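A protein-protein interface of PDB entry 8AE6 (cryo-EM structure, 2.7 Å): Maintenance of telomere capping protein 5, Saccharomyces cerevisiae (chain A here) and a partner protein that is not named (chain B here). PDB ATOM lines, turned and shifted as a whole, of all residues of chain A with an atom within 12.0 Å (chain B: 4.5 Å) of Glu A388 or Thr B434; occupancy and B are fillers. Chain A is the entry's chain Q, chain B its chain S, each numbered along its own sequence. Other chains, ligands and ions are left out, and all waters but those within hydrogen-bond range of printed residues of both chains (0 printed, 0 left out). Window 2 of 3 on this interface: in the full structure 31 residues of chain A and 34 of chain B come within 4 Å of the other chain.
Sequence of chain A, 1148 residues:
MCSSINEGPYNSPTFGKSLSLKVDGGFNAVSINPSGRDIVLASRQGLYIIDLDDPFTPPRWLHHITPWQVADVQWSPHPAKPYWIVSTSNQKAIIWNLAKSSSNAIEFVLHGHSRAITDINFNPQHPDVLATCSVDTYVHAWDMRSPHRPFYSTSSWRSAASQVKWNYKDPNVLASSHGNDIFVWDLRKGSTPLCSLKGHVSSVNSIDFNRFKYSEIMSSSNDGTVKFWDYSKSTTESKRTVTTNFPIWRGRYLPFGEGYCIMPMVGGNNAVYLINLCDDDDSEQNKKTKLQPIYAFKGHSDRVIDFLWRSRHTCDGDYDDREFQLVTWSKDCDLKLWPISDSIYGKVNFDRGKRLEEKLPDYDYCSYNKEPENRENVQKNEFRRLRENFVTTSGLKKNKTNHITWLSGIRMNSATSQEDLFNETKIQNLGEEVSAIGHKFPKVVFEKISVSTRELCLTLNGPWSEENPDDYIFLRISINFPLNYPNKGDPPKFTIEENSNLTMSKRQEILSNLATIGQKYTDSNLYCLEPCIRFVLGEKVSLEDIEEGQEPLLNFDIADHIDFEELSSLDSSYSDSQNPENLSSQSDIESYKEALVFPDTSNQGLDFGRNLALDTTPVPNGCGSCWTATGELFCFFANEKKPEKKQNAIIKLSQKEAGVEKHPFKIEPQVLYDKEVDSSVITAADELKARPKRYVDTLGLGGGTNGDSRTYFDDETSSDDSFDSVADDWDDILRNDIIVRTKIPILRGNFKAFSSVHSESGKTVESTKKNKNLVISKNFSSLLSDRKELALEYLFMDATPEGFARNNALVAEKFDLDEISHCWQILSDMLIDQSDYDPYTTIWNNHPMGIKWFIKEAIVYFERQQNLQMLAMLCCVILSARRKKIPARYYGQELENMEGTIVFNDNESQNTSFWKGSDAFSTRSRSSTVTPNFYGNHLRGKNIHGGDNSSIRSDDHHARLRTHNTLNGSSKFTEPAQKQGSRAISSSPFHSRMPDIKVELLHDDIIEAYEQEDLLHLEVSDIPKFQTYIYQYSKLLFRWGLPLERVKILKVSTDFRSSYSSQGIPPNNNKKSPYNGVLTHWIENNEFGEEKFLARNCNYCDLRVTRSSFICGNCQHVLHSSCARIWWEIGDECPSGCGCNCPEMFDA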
ATOM      1  N   PHE A 383     -35.513   9.361  -1.982  1.00  0.00           N
ATOM      2  CA  PHE A 383     -35.448   7.913  -1.899  1.00  0.00           C
ATOM      3  C   PHE A 383     -34.066   7.469  -1.428  1.00  0.00           C
ATOM      4  O   PHE A 383     -33.132   8.266  -1.305  1.00  0.00           O
ATOM      5  CB  PHE A 383     -35.781   7.287  -3.252  1.00  0.00           C
ATOM      6  CG  PHE A 383     -37.209   7.472  -3.671  1.00  0.00           C
ATOM      7  CD1 PHE A 383     -38.216   7.585  -2.725  1.00  0.00           C
ATOM      8  CD2 PHE A 383     -37.544   7.539  -5.014  1.00  0.00           C
ATOM      9  CE1 PHE A 383     -39.535   7.757  -3.110  1.00  0.00           C
ATOM     10  CE2 PHE A 383     -38.861   7.711  -5.405  1.00  0.00           C
ATOM     11  CZ  PHE A 383     -39.855   7.820  -4.453  1.00  0.00           C
ATOM     12  N   ARG A 384     -33.942   6.174  -1.161  1.00  0.00           N
ATOM     13  CA  ARG A 384     -32.688   5.623  -0.675  1.00  0.00           C
ATOM     14  C   ARG A 384     -31.741   5.355  -1.841  1.00  0.00           C
ATOM     15  O   ARG A 384     -32.085   5.527  -3.014  1.00  0.00           O
ATOM     16  CB  ARG A 384     -32.948   4.353   0.131  1.00  0.00           C
ATOM     17  CG  ARG A 384     -34.037   4.497   1.181  1.00  0.00           C
ATOM     18  CD  ARG A 384     -34.264   3.192   1.925  1.00  0.00           C
ATOM     19  NE  ARG A 384     -35.357   3.295   2.886  1.00  0.00           N
ATOM     20  CZ  ARG A 384     -35.759   2.306   3.674  1.00  0.00           C
ATOM     21  NH1 ARG A 384     -35.182   1.117   3.638  1.00  0.00           N
ATOM     22  NH2 ARG A 384     -36.768   2.516   4.515  1.00  0.00           N
ATOM     23  N   ARG A 385     -30.528   4.924  -1.513  1.00  0.00           N
ATOM     24  CA  ARG A 385     -29.492   4.650  -2.498  1.00  0.00           C
ATOM     25  C   ARG A 385     -29.052   3.200  -2.394  1.00  0.00           C
ATOM     26  O   ARG A 385     -28.832   2.686  -1.292  1.00  0.00           O
ATOM     27  CB  ARG A 385     -28.286   5.570  -2.299  1.00  0.00           C
ATOM     28  CG  ARG A 385     -28.524   6.999  -2.739  1.00  0.00           C
ATOM     29  CD  ARG A 385     -27.287   7.852  -2.552  1.00  0.00           C
ATOM     30  NE  ARG A 385     -27.589   9.268  -2.709  1.00  0.00           N
ATOM     31  CZ  ARG A 385     -26.704  10.243  -2.557  1.00  0.00           C
ATOM     32  NH1 ARG A 385     -25.446   9.989  -2.242  1.00  0.00           N
ATOM     33  NH2 ARG A 385     -27.093  11.504  -2.725  1.00  0.00           N
ATOM     34  N   LEU A 386     -28.928   2.545  -3.541  1.00  0.00           N
ATOM     35  CA  LEU A 386     -28.427   1.181  -3.568  1.00  0.00           C
ATOM     36  C   LEU A 386     -26.931   1.161  -3.276  1.00  0.00           C
ATOM     37  O   LEU A 386     -26.187   2.065  -3.665  1.00  0.00           O
ATOM     38  CB  LEU A 386     -28.704   0.535  -4.923  1.00  0.00           C
ATOM     39  CG  LEU A 386     -28.647  -0.991  -4.990  1.00  0.00           C
ATOM     40  CD1 LEU A 386     -29.627  -1.610  -4.005  1.00  0.00           C
ATOM     41  CD2 LEU A 386     -28.920  -1.479  -6.404  1.00  0.00           C
ATOM     42  N   ARG A 387     -26.495   0.120  -2.572  1.00  0.00           N
ATOM     43  CA  ARG A 387     -25.079  -0.039  -2.271  1.00  0.00           C
ATOM     44  C   ARG A 387     -24.338  -0.440  -3.539  1.00  0.00           C
ATOM     45  O   ARG A 387     -24.642  -1.473  -4.145  1.00  0.00           O
ATOM     46  CB  ARG A 387     -24.879  -1.086  -1.178  1.00  0.00           C
ATOM     47  CG  ARG A 387     -25.498  -0.719   0.160  1.00  0.00           C
ATOM     48  CD  ARG A 387     -25.291  -1.824   1.182  1.00  0.00           C
ATOM     49  NE  ARG A 387     -25.969  -1.539   2.441  1.00  0.00           N
ATOM     50  CZ  ARG A 387     -25.984  -2.357   3.486  1.00  0.00           C
ATOM     51  NH1 ARG A 387     -25.366  -3.527   3.457  1.00  0.00           N
ATOM     52  NH2 ARG A 387     -26.635  -1.993   4.587  1.00  0.00           N
ATOM     53  N   GLU A 388     -23.368   0.376  -3.939  1.00  0.00           N
ATOM     54  CA  GLU A 388     -22.679   0.165  -5.203  1.00  0.00           C
ATOM     55  C   GLU A 388     -21.249   0.667  -5.091  1.00  0.00           C
ATOM     56  O   GLU A 388     -20.955   1.597  -4.340  1.00  0.00           O
ATOM     57  CB  GLU A 388     -23.395   0.881  -6.350  1.00  0.00           C
ATOM     58  CG  GLU A 388     -23.756   2.324  -6.027  1.00  0.00           C
ATOM     59  CD  GLU A 388     -24.163   3.114  -7.248  1.00  0.00           C
ATOM     60  OE1 GLU A 388     -23.886   2.654  -8.373  1.00  0.00           O
ATOM     61  OE2 GLU A 388     -24.762   4.198  -7.084  1.00  0.00           O
ATOM     62  N   ASN A 389     -20.366   0.036  -5.853  1.00  0.00           N
ATOM     63  CA  ASN A 389     -18.992   0.493  -6.032  1.00  0.00           C
ATOM     64  C   ASN A 389     -18.915   0.994  -7.466  1.00  0.00           C
ATOM     65  O   ASN A 389     -18.672   0.229  -8.396  1.00  0.00           O
ATOM     66  CB  ASN A 389     -17.991  -0.622  -5.762  1.00  0.00           C
ATOM     67  CG  ASN A 389     -16.571  -0.112  -5.657  1.00  0.00           C
ATOM     68  OD1 ASN A 389     -16.343   1.083  -5.478  1.00  0.00           O
ATOM     69  ND2 ASN A 389     -15.608  -1.016  -5.769  1.00  0.00           N
ATOM     70  N   PHE A 390     -19.141   2.298  -7.638  1.00  0.00           N
ATOM     71  CA  PHE A 390     -19.291   2.870  -8.971  1.00  0.00           C
ATOM     72  C   PHE A 390     -17.962   2.904  -9.709  1.00  0.00           C
ATOM     73  O   PHE A 390     -17.807   2.289 -10.771  1.00  0.00           O
ATOM     74  CB  PHE A 390     -19.888   4.270  -8.857  1.00  0.00           C
ATOM     75  CG  PHE A 390     -19.975   5.006 -10.157  1.00  0.00           C
ATOM     76  CD1 PHE A 390     -20.568   4.419 -11.262  1.00  0.00           C
ATOM     77  CD2 PHE A 390     -19.491   6.293 -10.266  1.00  0.00           C
ATOM     78  CE1 PHE A 390     -20.652   5.100 -12.454  1.00  0.00           C
ATOM     79  CE2 PHE A 390     -19.579   6.979 -11.457  1.00  0.00           C
ATOM     80  CZ  PHE A 390     -20.166   6.382 -12.549  1.00  0.00           C
ATOM     81  N   VAL A 391     -16.987   3.619  -9.162  1.00  0.00           N
ATOM     82  CA  VAL A 391     -15.671   3.754  -9.764  1.00  0.00           C
ATOM     83  C   VAL A 391     -14.648   3.303  -8.735  1.00  0.00           C
ATOM     84  O   VAL A 391     -14.885   3.394  -7.526  1.00  0.00           O
ATOM     85  CB  VAL A 391     -15.423   5.206 -10.244  1.00  0.00           C
ATOM     86  CG1 VAL A 391     -15.317   6.182  -9.075  1.00  0.00           C
ATOM     87  CG2 VAL A 391     -14.217   5.300 -11.169  1.00  0.00           C
ATOM     88  N   THR A 392     -13.538   2.756  -9.213  1.00  0.00           N
ATOM     89  CA  THR A 392     -12.488   2.283  -8.325  1.00  0.00           C
ATOM     90  C   THR A 392     -11.801   3.456  -7.636  1.00  0.00           C
ATOM     91  O   THR A 392     -11.443   4.450  -8.270  1.00  0.00           O
ATOM     92  CB  THR A 392     -11.471   1.463  -9.112  1.00  0.00           C
ATOM     93  OG1 THR A 392     -12.153   0.439  -9.843  1.00  0.00           O
ATOM     94  CG2 THR A 392     -10.475   0.826  -8.178  1.00  0.00           C
ATOM     95  N   THR A 393     -11.629   3.332  -6.316  1.00  0.00           N
ATOM     96  CA  THR A 393     -10.949   4.366  -5.545  1.00  0.00           C
ATOM     97  C   THR A 393      -9.466   4.437  -5.899  1.00  0.00           C
ATOM     98  O   THR A 393      -8.885   5.531  -5.917  1.00  0.00           O
ATOM     99  CB  THR A 393     -11.153   4.100  -4.049  1.00  0.00           C
ATOM    100  OG1 THR A 393     -12.554   4.104  -3.756  1.00  0.00           O
ATOM    101  CG2 THR A 393     -10.484   5.168  -3.187  1.00  0.00           C
ATOM    102  N   LEU A 396      -8.471   6.867  -8.616  1.00  0.00           N
ATOM    103  CA  LEU A 396      -8.651   8.292  -8.363  1.00  0.00           C
ATOM    104  C   LEU A 396      -7.349   8.928  -7.888  1.00  0.00           C
ATOM    105  O   LEU A 396      -7.365   9.919  -7.159  1.00  0.00           O
ATOM    106  CB  LEU A 396      -9.755   8.516  -7.327  1.00  0.00           C
ATOM    107  CG  LEU A 396     -11.145   7.988  -7.686  1.00  0.00           C
ATOM    108  CD1 LEU A 396     -12.081   8.090  -6.497  1.00  0.00           C
ATOM    109  CD2 LEU A 396     -11.705   8.750  -8.870  1.00  0.00           C
ATOM    110  N   GLN B 335     -27.466  11.832  -8.677  1.00  0.00           N
ATOM    111  CA  GLN B 335     -28.518  10.957  -8.167  1.00  0.00           C
ATOM    112  C   GLN B 335     -29.563  11.747  -7.391  1.00  0.00           C
ATOM    113  O   GLN B 335     -30.771  11.548  -7.571  1.00  0.00           O
ATOM    114  CB  GLN B 335     -27.919   9.876  -7.272  1.00  0.00           C
ATOM    115  CG  GLN B 335     -27.050   8.873  -7.971  1.00  0.00           C
ATOM    116  CD  GLN B 335     -26.707   7.704  -7.082  1.00  0.00           C
ATOM    117  OE1 GLN B 335     -25.797   7.782  -6.260  1.00  0.00           O
ATOM    118  NE2 GLN B 335     -27.441   6.610  -7.233  1.00  0.00           N
ATOM    119  N   LEU B 432     -32.921   5.362  -5.675  1.00  0.00           N
ATOM    120  CA  LEU B 432     -32.396   6.319  -6.632  1.00  0.00           C
ATOM    121  C   LEU B 432     -31.720   5.586  -7.789  1.00  0.00           C
ATOM    122  O   LEU B 432     -31.267   4.448  -7.628  1.00  0.00           O
ATOM    123  CB  LEU B 432     -31.401   7.258  -5.958  1.00  0.00           C
ATOM    124  CG  LEU B 432     -31.984   8.346  -5.058  1.00  0.00           C
ATOM    125  CD1 LEU B 432     -30.886   9.252  -4.546  1.00  0.00           C
ATOM    126  CD2 LEU B 432     -33.032   9.143  -5.797  1.00  0.00           C
ATOM    127  N   PRO B 433     -31.678   6.198  -8.976  1.00  0.00           N
ATOM    128  CA  PRO B 433     -30.921   5.604 -10.085  1.00  0.00           C
ATOM    129  C   PRO B 433     -29.442   5.504  -9.761  1.00  0.00           C
ATOM    130  O   PRO B 433     -28.855   6.408  -9.165  1.00  0.00           O
ATOM    131  CB  PRO B 433     -31.174   6.575 -11.246  1.00  0.00           C
ATOM    132  CG  PRO B 433     -31.714   7.814 -10.618  1.00  0.00           C
ATOM    133  CD  PRO B 433     -32.469   7.352  -9.423  1.00  0.00           C
ATOM    134  N   THR B 434     -28.843   4.387 -10.154  1.00  0.00           N
ATOM    135  CA  THR B 434     -27.434   4.171  -9.898  1.00  0.00           C
ATOM    136  C   THR B 434     -26.588   5.080 -10.783  1.00  0.00           C
ATOM    137  O   THR B 434     -27.029   5.559 -11.833  1.00  0.00           O
ATOM    138  CB  THR B 434     -27.063   2.702 -10.118  1.00  0.00           C
ATOM    139  OG1 THR B 434     -25.656   2.523  -9.919  1.00  0.00           O
ATOM    140  CG2 THR B 434     -27.438   2.252 -11.516  1.00  0.00           C
ATOM    141  N   ARG B 435     -25.358   5.333 -10.329  1.00  0.00           N
ATOM    142  CA  ARG B 435     -24.468   6.238 -11.044  1.00  0.00           C
ATOM    143  C   ARG B 435     -24.026   5.653 -12.378  1.00  0.00           C
ATOM    144  O   ARG B 435     -23.719   6.405 -13.313  1.00  0.00           O
ATOM    145  CB  ARG B 435     -23.259   6.565 -10.173  1.00  0.00           C
ATOM    146  CG  ARG B 435     -23.617   6.881  -8.733  1.00  0.00           C
ATOM    147  CD  ARG B 435     -22.416   6.729  -7.820  1.00  0.00           C
ATOM    148  NE  ARG B 435     -22.673   7.253  -6.485  1.00  0.00           N
ATOM    149  CZ  ARG B 435     -22.501   6.564  -5.366  1.00  0.00           C
ATOM    150  NH1 ARG B 435     -22.067   5.318  -5.381  1.00  0.00           N
ATOM    151  NH2 ARG B 435     -22.774   7.145  -4.201  1.00  0.00           N
ATOM    152  N   SER B 436     -23.992   4.322 -12.483  1.00  0.00           N
ATOM    153  CA  SER B 436     -23.688   3.679 -13.756  1.00  0.00           C
ATOM    154  C   SER B 436     -24.771   3.961 -14.787  1.00  0.00           C
ATOM    155  O   SER B 436     -24.470   4.176 -15.966  1.00  0.00           O
ATOM    156  CB  SER B 436     -23.518   2.178 -13.549  1.00  0.00           C
ATOM    157  OG  SER B 436     -22.450   1.911 -12.657  1.00  0.00           O
ATOM    158  N   CYS B 437     -26.035   3.969 -14.357  1.00  0.00           N
ATOM    159  CA  CYS B 437     -27.135   4.313 -15.250  1.00  0.00           C
ATOM    160  C   CYS B 437     -27.017   5.746 -15.753  1.00  0.00           C
ATOM    161  O   CYS B 437     -27.225   6.013 -16.945  1.00  0.00           O
ATOM    162  CB  CYS B 437     -28.468   4.116 -14.532  1.00  0.00           C
ATOM    163  SG  CYS B 437     -29.910   4.562 -15.491  1.00  0.00           S
ATOM    164  N   LEU B 438     -26.667   6.673 -14.861  1.00  0.00           N
ATOM    165  CA  LEU B 438     -26.515   8.069 -15.253  1.00  0.00           C
ATOM    166  C   LEU B 438     -25.344   8.256 -16.207  1.00  0.00           C
ATOM    167  O   LEU B 438     -25.446   9.013 -17.181  1.00  0.00           O
ATOM    168  CB  LEU B 438     -26.345   8.940 -14.014  1.00  0.00           C
ATOM    169  CG  LEU B 438     -27.499   8.848 -13.019  1.00  0.00           C
ATOM    170  CD1 LEU B 438     -27.120   9.475 -11.693  1.00  0.00           C
ATOM    171  CD2 LEU B 438     -28.730   9.502 -13.593  1.00  0.00           C
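Of chain A, only Glu A388 comes within 4 Å of Thr B434.
Of chain A, only Phe A383 (3.9 Å), Arg A384 (2.8 Å) and Arg A385 (3.7 Å) come within 4 Å of Leu B432.
No residue of chain A comes within 4 Å of Pro B433.
Of chain A, only Glu A388 and Phe A390 come within 4 Å of Arg B435.
Ser B436 touches just one residue of chain A: Phe A390.
No residue of chain A comes within 4 Å of Cys B437.
No residue of chain A comes within 4 Å of Leu B438.
Of the printed residues of chain B, Phe A383 touches Leu B432.
Printed residues of chain A within 4 Å of Gln B335: Arg A385 and Glu A388.
Printed residues of chain B within 4 Å of Arg A385: Gln B335 and Leu B432.
Printed residues of chain B within 4 Å of Phe A390: Arg B435 (3.4 Å) and Ser B436 (3.4 Å).
Arg A387 touches none of the printed residues of chain B.
The backbone carbonyl oxygen (O) of Arg A384 sits at hydrogen-bond distance from the backbone NH (N) of Leu B432 (2.8 Å).
The side-chain carboxylate of Glu A388 sits close to the side-chain hydroxyl of Thr B434, 3.4 Å away.
OE2 of Glu A388 lies within salt-bridge range of NH1 of Arg B435.
Among the printed residues, pairs that only touch across the chains: Phe A383 with Leu B432 (3.9 Å), Arg A385 with Gln B335 (3.997 Å), Arg A385 with Leu B432 (3.7 Å), Glu A388 with Gln B335 (3.6 Å), Phe A390 with Arg B435 (3.4 Å) and Phe A390 with Ser B436 (3.4 Å).
Hydrophobic or aromatic side chains of chain A within 4 Å of the printed part of chain B: Phe A390.
Along chain A the printed residues that touch a printed residue of chain B span positions 383 to 390.
Of the 8 printed residues of chain B, 5 touch a printed residue of chain A.
NE2 of Gln B335 sits at hydrogen-bond distance from O of Pro B433 (2.4 Å).
The side-chain amide oxygen of Gln B335 lies within hydrogen-bond range of the guanidinium group of Arg B435 (3.2 Å).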
